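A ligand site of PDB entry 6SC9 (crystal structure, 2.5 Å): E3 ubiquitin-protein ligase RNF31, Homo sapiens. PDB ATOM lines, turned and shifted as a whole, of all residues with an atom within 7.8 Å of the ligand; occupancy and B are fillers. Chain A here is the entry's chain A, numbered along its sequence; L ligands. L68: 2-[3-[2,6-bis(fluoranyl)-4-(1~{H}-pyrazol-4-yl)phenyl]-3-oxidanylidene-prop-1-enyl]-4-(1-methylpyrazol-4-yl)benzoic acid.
The side-chain carboxylate (OD1) of Asp 240 is in hydrogen-bond range of a nitrogen (N31) of the ligand (2.9 Å). The backbone NH of Met 190 lies within hydrogen-bond range of an oxygen (O18) of the ligand (2.9 Å). The side-chain sulfur (SG) of Cys 189 is bonded to a carbon (C14) of the ligand. The guanidinium group (NH1) of Arg 239 is in salt-bridge range of an oxygen (O17) of the ligand, 2.9 Å away.
A ring nitrogen (NE2) of His 191 lies within hydrogen-bond range of the side-chain amide oxygen of Gln 200 (2.7 Å). O of Met 190 lies within hydrogen-bond range of N of Ser 203. O of Gly 188 is in hydrogen-bond range of NH2 of Arg 239. The guanidinium group (NE) of Arg 239 sits at hydrogen-bond distance from the backbone carbonyl oxygen (O) of Phe 236. The side-chain sulfur (SG) of Cys 189 sits close to the backbone NH (N) of His 191, at 3.6 Å.
Residues that only touch the ligand: Phe 236 (3.4 Å), His 191 (3.5 Å) and Leu 226 (3.95 Å). Hydrophobic or aromatic side chains that line the ligand: Met 190, His 191, Leu 226 and Phe 236. The nearest printed residue that does not touch the ligand is Phe 209 (4.02 Å).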
ATOM      1  N   GLY A 187       1.311  11.606  25.085  1.00  0.00           N
ATOM      2  CA  GLY A 187       0.945  12.673  24.179  1.00  0.00           C
ATOM      3  C   GLY A 187       1.867  12.770  22.975  1.00  0.00           C
ATOM      4  O   GLY A 187       2.431  11.775  22.517  1.00  0.00           O
ATOM      5  N   GLY A 188       2.016  13.989  22.463  1.00  0.00           N
ATOM      6  CA  GLY A 188       2.812  14.215  21.270  1.00  0.00           C
ATOM      7  C   GLY A 188       4.260  14.584  21.524  1.00  0.00           C
ATOM      8  O   GLY A 188       5.120  14.367  20.667  1.00  0.00           O
ATOM      9  N   CYS A 189       4.540  15.147  22.691  1.00  0.00           N
ATOM     10  CA  CYS A 189       5.876  15.588  23.074  1.00  0.00           C
ATOM     11  C   CYS A 189       6.440  14.664  24.138  1.00  0.00           C
ATOM     12  O   CYS A 189       5.747  14.349  25.117  1.00  0.00           O
ATOM     13  CB  CYS A 189       5.847  17.033  23.572  1.00  0.00           C
ATOM     14  SG  CYS A 189       7.408  17.677  24.231  1.00  0.00           S
ATOM     15  N   MET A 190       7.693  14.244  23.966  1.00  0.00           N
ATOM     16  CA  MET A 190       8.287  13.268  24.866  1.00  0.00           C
ATOM     17  C   MET A 190       8.898  13.874  26.113  1.00  0.00           C
ATOM     18  O   MET A 190       9.146  13.153  27.087  1.00  0.00           O
ATOM     19  CB  MET A 190       9.369  12.463  24.124  1.00  0.00           C
ATOM     20  CG  MET A 190       8.902  11.857  22.814  1.00  0.00           C
ATOM     21  SD  MET A 190       7.374  10.928  22.997  1.00  0.00           S
ATOM     22  CE  MET A 190       7.886   9.697  24.187  1.00  0.00           C
ATOM     23  N   HIS A 191       9.153  15.190  26.119  1.00  0.00           N
ATOM     24  CA  HIS A 191       9.798  15.810  27.273  1.00  0.00           C
ATOM     25  C   HIS A 191       8.845  15.855  28.460  1.00  0.00           C
ATOM     26  O   HIS A 191       7.689  16.273  28.340  1.00  0.00           O
ATOM     27  CB  HIS A 191      10.251  17.223  26.920  1.00  0.00           C
ATOM     28  CG  HIS A 191      11.002  17.908  28.032  1.00  0.00           C
ATOM     29  ND1 HIS A 191      10.393  18.772  28.908  1.00  0.00           N
ATOM     30  CD2 HIS A 191      12.306  17.839  28.398  1.00  0.00           C
ATOM     31  CE1 HIS A 191      11.294  19.219  29.770  1.00  0.00           C
ATOM     32  NE2 HIS A 191      12.455  18.666  29.477  1.00  0.00           N
ATOM     33  N   PHE A 192       9.327  15.412  29.622  1.00  0.00           N
ATOM     34  CA  PHE A 192       8.546  15.382  30.842  1.00  0.00           C
ATOM     35  C   PHE A 192       9.379  15.934  31.986  1.00  0.00           C
ATOM     36  O   PHE A 192      10.515  15.506  32.197  1.00  0.00           O
ATOM     37  CB  PHE A 192       8.086  13.959  31.176  1.00  0.00           C
ATOM     38  CG  PHE A 192       6.959  13.894  32.166  1.00  0.00           C
ATOM     39  CD1 PHE A 192       7.217  13.874  33.529  1.00  0.00           C
ATOM     40  CD2 PHE A 192       5.645  13.853  31.734  1.00  0.00           C
ATOM     41  CE1 PHE A 192       6.185  13.821  34.439  1.00  0.00           C
ATOM     42  CE2 PHE A 192       4.607  13.802  32.651  1.00  0.00           C
ATOM     43  CZ  PHE A 192       4.878  13.779  33.999  1.00  0.00           C
ATOM     44  N   HIS A 193       8.823  16.903  32.711  1.00  0.00           N
ATOM     45  CA  HIS A 193       9.478  17.513  33.862  1.00  0.00           C
ATOM     46  C   HIS A 193       8.702  17.114  35.109  1.00  0.00           C
ATOM     47  O   HIS A 193       7.524  17.463  35.254  1.00  0.00           O
ATOM     48  CB  HIS A 193       9.530  19.034  33.715  1.00  0.00           C
ATOM     49  CG  HIS A 193      10.442  19.697  34.703  1.00  0.00           C
ATOM     50  ND1 HIS A 193      11.755  19.997  34.421  1.00  0.00           N
ATOM     51  CD2 HIS A 193      10.225  20.128  35.973  1.00  0.00           C
ATOM     52  CE1 HIS A 193      12.314  20.570  35.468  1.00  0.00           C
ATOM     53  NE2 HIS A 193      11.407  20.662  36.430  1.00  0.00           N
ATOM     54  N   GLN A 200      14.267  15.821  34.327  1.00  0.00           N
ATOM     55  CA  GLN A 200      13.849  15.934  32.938  1.00  0.00           C
ATOM     56  C   GLN A 200      14.228  14.650  32.217  1.00  0.00           C
ATOM     57  O   GLN A 200      15.415  14.323  32.115  1.00  0.00           O
ATOM     58  CB  GLN A 200      14.493  17.147  32.270  1.00  0.00           C
ATOM     59  CG  GLN A 200      14.342  18.430  33.058  1.00  0.00           C
ATOM     60  CD  GLN A 200      14.563  19.668  32.214  1.00  0.00           C
ATOM     61  OE1 GLN A 200      14.446  19.627  30.988  1.00  0.00           O
ATOM     62  NE2 GLN A 200      14.862  20.785  32.866  1.00  0.00           N
ATOM     63  N   CYS A 202      12.724  11.468  29.113  1.00  0.00           N
ATOM     64  CA  CYS A 202      11.801  11.098  28.054  1.00  0.00           C
ATOM     65  C   CYS A 202      10.734  10.175  28.614  1.00  0.00           C
ATOM     66  O   CYS A 202      11.043   9.199  29.303  1.00  0.00           O
ATOM     67  CB  CYS A 202      12.558  10.423  26.906  1.00  0.00           C
ATOM     68  SG  CYS A 202      11.505   9.847  25.559  1.00  0.00           S
ATOM     69  N   SER A 203       9.467  10.479  28.326  1.00  0.00           N
ATOM     70  CA  SER A 203       8.366   9.674  28.818  1.00  0.00           C
ATOM     71  C   SER A 203       8.200   8.354  28.056  1.00  0.00           C
ATOM     72  O   SER A 203       7.375   7.526  28.458  1.00  0.00           O
ATOM     73  CB  SER A 203       7.056  10.460  28.757  1.00  0.00           C
ATOM     74  OG  SER A 203       6.729  10.812  27.426  1.00  0.00           O
ATOM     75  N   PHE A 209      17.077  13.765  29.972  1.00  0.00           N
ATOM     76  CA  PHE A 209      17.280  14.910  29.079  1.00  0.00           C
ATOM     77  C   PHE A 209      18.397  15.755  29.671  1.00  0.00           C
ATOM     78  O   PHE A 209      18.191  16.492  30.631  1.00  0.00           O
ATOM     79  CB  PHE A 209      16.003  15.712  28.908  1.00  0.00           C
ATOM     80  CG  PHE A 209      15.213  15.358  27.680  1.00  0.00           C
ATOM     81  CD1 PHE A 209      14.258  14.340  27.725  1.00  0.00           C
ATOM     82  CD2 PHE A 209      15.402  16.034  26.494  1.00  0.00           C
ATOM     83  CE1 PHE A 209      13.528  14.014  26.598  1.00  0.00           C
ATOM     84  CE2 PHE A 209      14.677  15.715  25.356  1.00  0.00           C
ATOM     85  CZ  PHE A 209      13.736  14.706  25.412  1.00  0.00           C
ATOM     86  N   LEU A 226      19.987  21.156  25.047  1.00  0.00           N
ATOM     87  CA  LEU A 226      19.079  20.276  25.765  1.00  0.00           C
ATOM     88  C   LEU A 226      18.632  19.155  24.834  1.00  0.00           C
ATOM     89  O   LEU A 226      18.049  19.412  23.770  1.00  0.00           O
ATOM     90  CB  LEU A 226      17.881  21.060  26.274  1.00  0.00           C
ATOM     91  CG  LEU A 226      16.987  20.507  27.395  1.00  0.00           C
ATOM     92  CD1 LEU A 226      15.976  19.502  26.861  1.00  0.00           C
ATOM     93  CD2 LEU A 226      17.802  19.901  28.519  1.00  0.00           C
ATOM     94  N   HIS A 227      18.902  17.903  25.223  1.00  0.00           N
ATOM     95  CA  HIS A 227      18.584  16.771  24.369  1.00  0.00           C
ATOM     96  C   HIS A 227      18.639  15.486  25.196  1.00  0.00           C
ATOM     97  O   HIS A 227      19.074  15.487  26.346  1.00  0.00           O
ATOM     98  CB  HIS A 227      19.533  16.667  23.177  1.00  0.00           C
ATOM     99  CG  HIS A 227      20.918  16.242  23.553  1.00  0.00           C
ATOM    100  ND1 HIS A 227      21.778  17.039  24.266  1.00  0.00           N
ATOM    101  CD2 HIS A 227      21.590  15.081  23.320  1.00  0.00           C
ATOM    102  CE1 HIS A 227      22.923  16.398  24.448  1.00  0.00           C
ATOM    103  NE2 HIS A 227      22.831  15.217  23.884  1.00  0.00           N
ATOM    104  N   GLY A 228      18.186  14.399  24.577  1.00  0.00           N
ATOM    105  CA  GLY A 228      18.294  13.078  25.161  1.00  0.00           C
ATOM    106  C   GLY A 228      18.676  12.058  24.118  1.00  0.00           C
ATOM    107  O   GLY A 228      18.729  12.354  22.917  1.00  0.00           O
ATOM    108  N   HIS A 230      17.717   8.223  22.733  1.00  0.00           N
ATOM    109  CA  HIS A 230      16.583   7.312  22.746  1.00  0.00           C
ATOM    110  C   HIS A 230      16.920   6.034  21.986  1.00  0.00           C
ATOM    111  O   HIS A 230      17.556   6.098  20.929  1.00  0.00           O
ATOM    112  CB  HIS A 230      15.345   7.962  22.129  1.00  0.00           C
ATOM    113  CG  HIS A 230      15.117   9.375  22.567  1.00  0.00           C
ATOM    114  ND1 HIS A 230      14.133   9.732  23.460  1.00  0.00           N
ATOM    115  CD2 HIS A 230      15.738  10.529  22.214  1.00  0.00           C
ATOM    116  CE1 HIS A 230      14.168  11.038  23.652  1.00  0.00           C
ATOM    117  NE2 HIS A 230      15.124  11.546  22.906  1.00  0.00           N
ATOM    118  N   LEU A 235       9.112   5.857  21.531  1.00  0.00           N
ATOM    119  CA  LEU A 235       8.107   6.704  20.890  1.00  0.00           C
ATOM    120  C   LEU A 235       8.709   7.983  20.319  1.00  0.00           C
ATOM    121  O   LEU A 235       8.139   8.559  19.389  1.00  0.00           O
ATOM    122  CB  LEU A 235       6.999   7.033  21.895  1.00  0.00           C
ATOM    123  CG  LEU A 235       5.863   7.964  21.472  1.00  0.00           C
ATOM    124  CD1 LEU A 235       5.166   7.426  20.229  1.00  0.00           C
ATOM    125  CD2 LEU A 235       4.876   8.148  22.614  1.00  0.00           C
ATOM    126  N   PHE A 236       9.853   8.424  20.843  1.00  0.00           N
ATOM    127  CA  PHE A 236      10.506   9.619  20.308  1.00  0.00           C
ATOM    128  C   PHE A 236      10.812   9.467  18.829  1.00  0.00           C
ATOM    129  O   PHE A 236      10.748  10.444  18.073  1.00  0.00           O
ATOM    130  CB  PHE A 236      11.800   9.899  21.091  1.00  0.00           C
ATOM    131  CG  PHE A 236      12.552  11.111  20.612  1.00  0.00           C
ATOM    132  CD1 PHE A 236      12.237  12.375  21.098  1.00  0.00           C
ATOM    133  CD2 PHE A 236      13.580  10.991  19.695  1.00  0.00           C
ATOM    134  CE1 PHE A 236      12.927  13.491  20.666  1.00  0.00           C
ATOM    135  CE2 PHE A 236      14.284  12.109  19.261  1.00  0.00           C
ATOM    136  CZ  PHE A 236      13.951  13.358  19.748  1.00  0.00           C
ATOM    137  N   TYR A 237      11.136   8.255  18.381  1.00  0.00           N
ATOM    138  CA  TYR A 237      11.389   7.955  16.981  1.00  0.00           C
ATOM    139  C   TYR A 237      10.180   7.370  16.268  1.00  0.00           C
ATOM    140  O   TYR A 237       9.908   7.726  15.119  1.00  0.00           O
ATOM    141  CB  TYR A 237      12.576   6.987  16.851  1.00  0.00           C
ATOM    142  CG  TYR A 237      13.909   7.611  17.167  1.00  0.00           C
ATOM    143  CD1 TYR A 237      14.383   8.682  16.432  1.00  0.00           C
ATOM    144  CD2 TYR A 237      14.709   7.112  18.189  1.00  0.00           C
ATOM    145  CE1 TYR A 237      15.617   9.264  16.709  1.00  0.00           C
ATOM    146  CE2 TYR A 237      15.942   7.678  18.482  1.00  0.00           C
ATOM    147  CZ  TYR A 237      16.383   8.756  17.730  1.00  0.00           C
ATOM    148  OH  TYR A 237      17.612   9.324  18.006  1.00  0.00           O
ATOM    149  N   ARG A 239       7.129   7.936  16.702  1.00  0.00           N
ATOM    150  CA  ARG A 239       6.068   8.903  16.445  1.00  0.00           C
ATOM    151  C   ARG A 239       6.160   9.460  15.023  1.00  0.00           C
ATOM    152  O   ARG A 239       5.154   9.911  14.476  1.00  0.00           O
ATOM    153  CB  ARG A 239       6.122  10.045  17.456  1.00  0.00           C
ATOM    154  CG  ARG A 239       7.368  10.910  17.349  1.00  0.00           C
ATOM    155  CD  ARG A 239       7.392  11.990  18.413  1.00  0.00           C
ATOM    156  NE  ARG A 239       8.677  12.699  18.413  1.00  0.00           N
ATOM    157  CZ  ARG A 239       8.964  13.728  19.207  1.00  0.00           C
ATOM    158  NH1 ARG A 239      10.157  14.305  19.139  1.00  0.00           N
ATOM    159  NH2 ARG A 239       8.050  14.177  20.062  1.00  0.00           N
ATOM    160  N   ASP A 240       7.354   9.438  14.434  1.00  0.00           N
ATOM    161  CA  ASP A 240       7.546   9.899  13.065  1.00  0.00           C
ATOM    162  C   ASP A 240       7.161   8.859  12.025  1.00  0.00           C
ATOM    163  O   ASP A 240       7.056   9.189  10.840  1.00  0.00           O
ATOM    164  CB  ASP A 240       9.001  10.330  12.840  1.00  0.00           C
ATOM    165  CG  ASP A 240       9.371  11.563  13.638  1.00  0.00           C
ATOM    166  OD1 ASP A 240       8.469  12.395  13.900  1.00  0.00           O
ATOM    167  OD2 ASP A 240      10.556  11.714  13.989  1.00  0.00           O
HETATM  168  C10 L68 L   1      10.530  17.652  22.913  1.00  0.00           C
HETATM  169  C13 L68 L   1      10.198  16.520  21.966  1.00  0.00           C
HETATM  170  C15 L68 L   1       7.468  19.898  22.626  1.00  0.00           C
HETATM  171  C21 L68 L   1       6.771  18.413  19.706  1.00  0.00           C
HETATM  172  C22 L68 L   1       7.017  17.460  18.717  1.00  0.00           C
HETATM  173  C24 L68 L   1       9.351  18.132  18.516  1.00  0.00           C
HETATM  174  C28 L68 L   1       8.496  16.295  17.092  1.00  0.00           C
HETATM  175  C01 L68 L   1      10.686  21.362  26.595  1.00  0.00           C
HETATM  176  C04 L68 L   1      12.751  21.471  25.706  1.00  0.00           C
HETATM  177  C05 L68 L   1      11.523  20.825  25.636  1.00  0.00           C
HETATM  178  C06 L68 L   1      11.100  23.234  28.337  1.00  0.00           C
HETATM  179  C07 L68 L   1      11.153  19.739  24.686  1.00  0.00           C
HETATM  180  C08 L68 L   1       9.852  19.637  24.211  1.00  0.00           C
HETATM  181  C09 L68 L   1       9.498  18.628  23.326  1.00  0.00           C
HETATM  182  C11 L68 L   1      11.823  17.775  23.418  1.00  0.00           C
HETATM  183  C12 L68 L   1      12.127  18.812  24.293  1.00  0.00           C
HETATM  184  C14 L68 L   1       8.072  18.521  22.836  1.00  0.00           C
HETATM  185  C16 L68 L   1       7.677  20.338  21.196  1.00  0.00           C
HETATM  186  C19 L68 L   1       7.879  19.296  20.134  1.00  0.00           C
HETATM  187  C23 L68 L   1       8.279  17.327  18.144  1.00  0.00           C
HETATM  188  C25 L68 L   1       9.206  19.117  19.492  1.00  0.00           C
HETATM  189  C29 L68 L   1       9.690  16.038  16.430  1.00  0.00           C
HETATM  190  C32 L68 L   1       7.541  15.406  16.612  1.00  0.00           C
HETATM  191  F26 L68 L   1       5.553  18.524  20.256  1.00  0.00           F
HETATM  192  F27 L68 L   1      10.254  19.881  19.837  1.00  0.00           F
HETATM  193  N02 L68 L   1      11.404  22.298  27.222  1.00  0.00           N
HETATM  194  N03 L68 L   1      12.693  22.393  26.691  1.00  0.00           N
HETATM  195  N30 L68 L   1       9.476  15.028  15.562  1.00  0.00           N
HETATM  196  N31 L68 L   1       8.130  14.632  15.672  1.00  0.00           N
HETATM  197  O17 L68 L   1      11.011  16.244  21.053  1.00  0.00           O
HETATM  198  O18 L68 L   1       9.132  15.879  22.117  1.00  0.00           O
HETATM  199  O20 L68 L   1       7.667  21.520  20.903  1.00  0.00           O
